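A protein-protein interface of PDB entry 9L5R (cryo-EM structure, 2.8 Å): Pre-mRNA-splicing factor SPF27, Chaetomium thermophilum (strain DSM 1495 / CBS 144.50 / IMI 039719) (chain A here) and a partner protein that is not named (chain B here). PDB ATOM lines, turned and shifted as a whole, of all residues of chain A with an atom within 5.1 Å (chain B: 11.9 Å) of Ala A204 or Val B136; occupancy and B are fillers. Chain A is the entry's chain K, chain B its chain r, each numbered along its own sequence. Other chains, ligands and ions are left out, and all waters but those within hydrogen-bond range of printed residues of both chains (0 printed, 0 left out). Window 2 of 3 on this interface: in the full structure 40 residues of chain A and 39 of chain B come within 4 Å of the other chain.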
ATOM      1  N   VAL A 199      11.999  -6.460   5.804  1.00  0.00           N
ATOM      2  CA  VAL A 199      11.102  -7.572   6.099  1.00  0.00           C
ATOM      3  C   VAL A 199      10.004  -7.136   7.060  1.00  0.00           C
ATOM      4  O   VAL A 199       8.877  -7.638   6.979  1.00  0.00           O
ATOM      5  CB  VAL A 199      11.890  -8.801   6.607  1.00  0.00           C
ATOM      6  CG1 VAL A 199      12.366  -8.640   8.042  1.00  0.00           C
ATOM      7  CG2 VAL A 199      11.058 -10.066   6.445  1.00  0.00           C
ATOM      8  N   LEU A 200      10.282  -6.171   7.944  1.00  0.00           N
ATOM      9  CA  LEU A 200       9.224  -5.648   8.801  1.00  0.00           C
ATOM     10  C   LEU A 200       8.180  -4.891   7.989  1.00  0.00           C
ATOM     11  O   LEU A 200       6.972  -5.100   8.167  1.00  0.00           O
ATOM     12  CB  LEU A 200       9.815  -4.761   9.896  1.00  0.00           C
ATOM     13  CG  LEU A 200      10.071  -5.409  11.262  1.00  0.00           C
ATOM     14  CD1 LEU A 200       8.750  -5.789  11.895  1.00  0.00           C
ATOM     15  CD2 LEU A 200      10.975  -6.628  11.186  1.00  0.00           C
ATOM     16  N   GLU A 201       8.629  -4.029   7.068  1.00  0.00           N
ATOM     17  CA  GLU A 201       7.686  -3.318   6.203  1.00  0.00           C
ATOM     18  C   GLU A 201       6.916  -4.286   5.312  1.00  0.00           C
ATOM     19  O   GLU A 201       5.704  -4.124   5.100  1.00  0.00           O
ATOM     20  CB  GLU A 201       8.424  -2.286   5.355  1.00  0.00           C
ATOM     21  CG  GLU A 201       9.051  -1.161   6.154  1.00  0.00           C
ATOM     22  CD  GLU A 201       9.856  -0.212   5.289  1.00  0.00           C
ATOM     23  OE1 GLU A 201       9.921  -0.436   4.063  1.00  0.00           O
ATOM     24  OE2 GLU A 201      10.429   0.752   5.836  1.00  0.00           O
ATOM     25  N   THR A 202       7.608  -5.302   4.791  1.00  0.00           N
ATOM     26  CA  THR A 202       6.993  -6.312   3.939  1.00  0.00           C
ATOM     27  C   THR A 202       5.900  -7.073   4.672  1.00  0.00           C
ATOM     28  O   THR A 202       4.798  -7.253   4.145  1.00  0.00           O
ATOM     29  CB  THR A 202       8.067  -7.279   3.440  1.00  0.00           C
ATOM     30  OG1 THR A 202       8.996  -6.582   2.601  1.00  0.00           O
ATOM     31  CG2 THR A 202       7.450  -8.446   2.699  1.00  0.00           C
ATOM     32  N   GLU A 203       6.181  -7.518   5.897  1.00  0.00           N
ATOM     33  CA  GLU A 203       5.171  -8.268   6.627  1.00  0.00           C
ATOM     34  C   GLU A 203       4.045  -7.367   7.111  1.00  0.00           C
ATOM     35  O   GLU A 203       2.914  -7.833   7.251  1.00  0.00           O
ATOM     36  CB  GLU A 203       5.807  -9.027   7.787  1.00  0.00           C
ATOM     37  CG  GLU A 203       6.436 -10.343   7.362  1.00  0.00           C
ATOM     38  CD  GLU A 203       6.959 -11.147   8.530  1.00  0.00           C
ATOM     39  OE1 GLU A 203       6.918 -10.636   9.668  1.00  0.00           O
ATOM     40  OE2 GLU A 203       7.408 -12.291   8.311  1.00  0.00           O
ATOM     41  N   ALA A 204       4.313  -6.073   7.319  1.00  0.00           N
ATOM     42  CA  ALA A 204       3.227  -5.146   7.628  1.00  0.00           C
ATOM     43  C   ALA A 204       2.276  -4.993   6.444  1.00  0.00           C
ATOM     44  O   ALA A 204       1.046  -5.068   6.600  1.00  0.00           O
ATOM     45  CB  ALA A 204       3.797  -3.789   8.037  1.00  0.00           C
ATOM     46  N   ALA A 205       2.830  -4.793   5.246  1.00  0.00           N
ATOM     47  CA  ALA A 205       1.995  -4.684   4.053  1.00  0.00           C
ATOM     48  C   ALA A 205       1.278  -5.996   3.756  1.00  0.00           C
ATOM     49  O   ALA A 205       0.116  -5.995   3.332  1.00  0.00           O
ATOM     50  CB  ALA A 205       2.841  -4.250   2.858  1.00  0.00           C
ATOM     51  N   ALA A 206       1.953  -7.125   3.986  1.00  0.00           N
ATOM     52  CA  ALA A 206       1.330  -8.427   3.792  1.00  0.00           C
ATOM     53  C   ALA A 206       0.211  -8.669   4.793  1.00  0.00           C
ATOM     54  O   ALA A 206      -0.798  -9.285   4.445  1.00  0.00           O
ATOM     55  CB  ALA A 206       2.381  -9.531   3.892  1.00  0.00           C
ATOM     56  N   GLU A 207       0.363  -8.190   6.029  1.00  0.00           N
ATOM     57  CA  GLU A 207      -0.712  -8.294   7.009  1.00  0.00           C
ATOM     58  C   GLU A 207      -1.903  -7.435   6.610  1.00  0.00           C
ATOM     59  O   GLU A 207      -3.057  -7.840   6.790  1.00  0.00           O
ATOM     60  CB  GLU A 207      -0.197  -7.890   8.390  1.00  0.00           C
ATOM     61  CG  GLU A 207      -0.890  -8.585   9.548  1.00  0.00           C
ATOM     62  CD  GLU A 207      -0.376  -9.992   9.773  1.00  0.00           C
ATOM     63  OE1 GLU A 207       0.744 -10.298   9.313  1.00  0.00           O
ATOM     64  OE2 GLU A 207      -1.086 -10.791  10.419  1.00  0.00           O
ATOM     65  N   LYS A 208      -1.642  -6.245   6.061  1.00  0.00           N
ATOM     66  CA  LYS A 208      -2.736  -5.408   5.572  1.00  0.00           C
ATOM     67  C   LYS A 208      -3.484  -6.095   4.431  1.00  0.00           C
ATOM     68  O   LYS A 208      -4.721  -6.181   4.442  1.00  0.00           O
ATOM     69  CB  LYS A 208      -2.193  -4.049   5.132  1.00  0.00           C
ATOM     70  CG  LYS A 208      -3.263  -3.013   4.835  1.00  0.00           C
ATOM     71  CD  LYS A 208      -3.448  -2.813   3.343  1.00  0.00           C
ATOM     72  CE  LYS A 208      -2.187  -2.273   2.699  1.00  0.00           C
ATOM     73  NZ  LYS A 208      -2.354  -2.124   1.229  1.00  0.00           N
ATOM     74  N   ALA B 130      16.140 -12.791  18.569  1.00  0.00           N
ATOM     75  CA  ALA B 130      14.745 -12.460  18.830  1.00  0.00           C
ATOM     76  C   ALA B 130      14.258 -11.347  17.911  1.00  0.00           C
ATOM     77  O   ALA B 130      13.145 -11.420  17.378  1.00  0.00           O
ATOM     78  CB  ALA B 130      14.564 -12.065  20.295  1.00  0.00           C
ATOM     79  N   LEU B 131      15.077 -10.311  17.710  1.00  0.00           N
ATOM     80  CA  LEU B 131      14.673  -9.233  16.816  1.00  0.00           C
ATOM     81  C   LEU B 131      14.699  -9.670  15.357  1.00  0.00           C
ATOM     82  O   LEU B 131      13.973  -9.098  14.539  1.00  0.00           O
ATOM     83  CB  LEU B 131      15.565  -8.008  17.047  1.00  0.00           C
ATOM     84  CG  LEU B 131      15.215  -6.649  16.428  1.00  0.00           C
ATOM     85  CD1 LEU B 131      15.686  -5.544  17.352  1.00  0.00           C
ATOM     86  CD2 LEU B 131      15.846  -6.454  15.060  1.00  0.00           C
ATOM     87  N   ALA B 132      15.500 -10.683  15.019  1.00  0.00           N
ATOM     88  CA  ALA B 132      15.540 -11.165  13.643  1.00  0.00           C
ATOM     89  C   ALA B 132      14.289 -11.954  13.280  1.00  0.00           C
ATOM     90  O   ALA B 132      13.917 -12.012  12.103  1.00  0.00           O
ATOM     91  CB  ALA B 132      16.788 -12.018  13.424  1.00  0.00           C
ATOM     92  N   ARG B 133      13.631 -12.569  14.264  1.00  0.00           N
ATOM     93  CA  ARG B 133      12.404 -13.319  14.032  1.00  0.00           C
ATOM     94  C   ARG B 133      11.165 -12.552  14.470  1.00  0.00           C
ATOM     95  O   ARG B 133      10.112 -13.160  14.687  1.00  0.00           O
ATOM     96  CB  ARG B 133      12.463 -14.673  14.741  1.00  0.00           C
ATOM     97  CG  ARG B 133      13.758 -15.438  14.535  1.00  0.00           C
ATOM     98  CD  ARG B 133      13.780 -16.190  13.210  1.00  0.00           C
ATOM     99  NE  ARG B 133      14.138 -15.334  12.084  1.00  0.00           N
ATOM    100  CZ  ARG B 133      15.363 -14.903  11.820  1.00  0.00           C
ATOM    101  NH1 ARG B 133      16.400 -15.267  12.558  1.00  0.00           N
ATOM    102  NH2 ARG B 133      15.558 -14.097  10.781  1.00  0.00           N
ATOM    103  N   LEU B 134      11.271 -11.236  14.605  1.00  0.00           N
ATOM    104  CA  LEU B 134      10.151 -10.416  15.054  1.00  0.00           C
ATOM    105  C   LEU B 134       9.145 -10.290  13.918  1.00  0.00           C
ATOM    106  O   LEU B 134       9.309  -9.474  13.010  1.00  0.00           O
ATOM    107  CB  LEU B 134      10.651  -9.051  15.511  1.00  0.00           C
ATOM    108  CG  LEU B 134       9.638  -8.087  16.129  1.00  0.00           C
ATOM    109  CD1 LEU B 134       8.686  -8.810  17.072  1.00  0.00           C
ATOM    110  CD2 LEU B 134      10.380  -6.996  16.874  1.00  0.00           C
ATOM    111  N   THR B 135       8.094 -11.102  13.970  1.00  0.00           N
ATOM    112  CA  THR B 135       7.049 -11.066  12.962  1.00  0.00           C
ATOM    113  C   THR B 135       6.119  -9.880  13.201  1.00  0.00           C
ATOM    114  O   THR B 135       6.214  -9.168  14.205  1.00  0.00           O
ATOM    115  CB  THR B 135       6.246 -12.365  12.965  1.00  0.00           C
ATOM    116  OG1 THR B 135       5.468 -12.442  14.166  1.00  0.00           O
ATOM    117  CG2 THR B 135       7.174 -13.567  12.898  1.00  0.00           C
ATOM    118  N   VAL B 136       5.206  -9.669  12.261  1.00  0.00           N
ATOM    119  CA  VAL B 136       4.200  -8.622  12.368  1.00  0.00           C
ATOM    120  C   VAL B 136       2.862  -9.287  12.646  1.00  0.00           C
ATOM    121  O   VAL B 136       2.341 -10.035  11.811  1.00  0.00           O
ATOM    122  CB  VAL B 136       4.135  -7.760  11.101  1.00  0.00           C
ATOM    123  CG1 VAL B 136       3.009  -6.747  11.217  1.00  0.00           C
ATOM    124  CG2 VAL B 136       5.451  -7.054  10.885  1.00  0.00           C
ATOM    125  N   THR B 137       2.305  -9.018  13.822  1.00  0.00           N
ATOM    126  CA  THR B 137       0.961  -9.467  14.138  1.00  0.00           C
ATOM    127  C   THR B 137      -0.062  -8.540  13.488  1.00  0.00           C
ATOM    128  O   THR B 137       0.260  -7.445  13.017  1.00  0.00           O
ATOM    129  CB  THR B 137       0.751  -9.516  15.650  1.00  0.00           C
ATOM    130  OG1 THR B 137       0.936  -8.206  16.201  1.00  0.00           O
ATOM    131  CG2 THR B 137       1.741 -10.476  16.292  1.00  0.00           C
ATOM    132  N   GLY B 138      -1.309  -8.999  13.453  1.00  0.00           N
ATOM    133  CA  GLY B 138      -2.390  -8.185  12.933  1.00  0.00           C
ATOM    134  C   GLY B 138      -2.646  -6.965  13.793  1.00  0.00           C
ATOM    135  O   GLY B 138      -3.115  -7.087  14.928  1.00  0.00           O
ATOM    136  N   ALA B 139      -2.337  -5.780  13.263  1.00  0.00           N
ATOM    137  CA  ALA B 139      -2.485  -4.530  14.009  1.00  0.00           C
ATOM    138  C   ALA B 139      -3.968  -4.177  14.078  1.00  0.00           C
ATOM    139  O   ALA B 139      -4.481  -3.328  13.345  1.00  0.00           O
ATOM    140  CB  ALA B 139      -1.668  -3.417  13.366  1.00  0.00           C
ATOM    141  N   ALA B 140      -4.665  -4.854  14.983  1.00  0.00           N
ATOM    142  CA  ALA B 140      -6.099  -4.650  15.131  1.00  0.00           C
ATOM    143  C   ALA B 140      -6.369  -3.341  15.864  1.00  0.00           C
ATOM    144  O   ALA B 140      -5.788  -3.103  16.930  1.00  0.00           O
ATOM    145  CB  ALA B 140      -6.729  -5.818  15.885  1.00  0.00           C
ATOM    146  N   PRO B 141      -7.218  -2.468  15.327  1.00  0.00           N
ATOM    147  CA  PRO B 141      -7.567  -1.239  16.048  1.00  0.00           C
ATOM    148  C   PRO B 141      -8.401  -1.534  17.285  1.00  0.00           C
ATOM    149  O   PRO B 141      -9.113  -2.538  17.362  1.00  0.00           O
ATOM    150  CB  PRO B 141      -8.367  -0.436  15.015  1.00  0.00           C
ATOM    151  CG  PRO B 141      -8.918  -1.465  14.086  1.00  0.00           C
ATOM    152  CD  PRO B 141      -7.888  -2.556  14.018  1.00  0.00           C
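Of chain B, only Val B136 (3.9 Å) comes within 4 Å of Ala A204. Printed residues of chain B within 4 Å of Leu A200: Leu B134 and Val B136. No residue of chain B comes within 4 Å of Thr A202. Printed residues of chain B within 4 Å of Glu A203: Thr B135 and Val B136. Ala A205 touches none of the printed residues of chain B. Of chain B, only Val B136 (3.0 Å), Thr B137 (3.8 Å) and Gly B138 (3.5 Å) come within 4 Å of Glu A207. No residue of chain B comes within 4 Å of Lys A208. Of the printed residues of chain A, Leu B134 touches Leu A200 (3.8 Å). Of the printed residues of chain A, Gly B138 touches Glu A207 (3.5 Å). Ala B139 touches none of the printed residues of chain A. Leu B131 touches none of the printed residues of chain A. The nearest printed residue of chain A that does not touch Val B136 is Val A199 (5.2 Å).
The backbone carbonyl oxygen (O) of Val B136 lies close to the side-chain carboxylate (OE1) of Glu A207 (3.0 Å). The side-chain carboxylate of Glu A203 is in hydrogen-bond range of the backbone NH of Val B136.
Of the 12 printed residues of chain B, 5 touch a printed residue of chain A. Hydrophobic or aromatic side chains of chain B that line the printed part of chain A: Val B136. Hydrophobic or aromatic side chains of chain A within 4 Å of the printed part of chain B: Leu A200.
Among the printed residues, merely in contact across the chains: Glu A203 with Thr B135 (3.3 Å), Glu A207 with Gly B138 (3.5 Å), Leu A200 with Val B136 (3.7 Å), Leu A200 with Leu B134 (3.8 Å), Glu A207 with Thr B137 (3.8 Å) and Ala A204 with Val B136 (3.9 Å).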
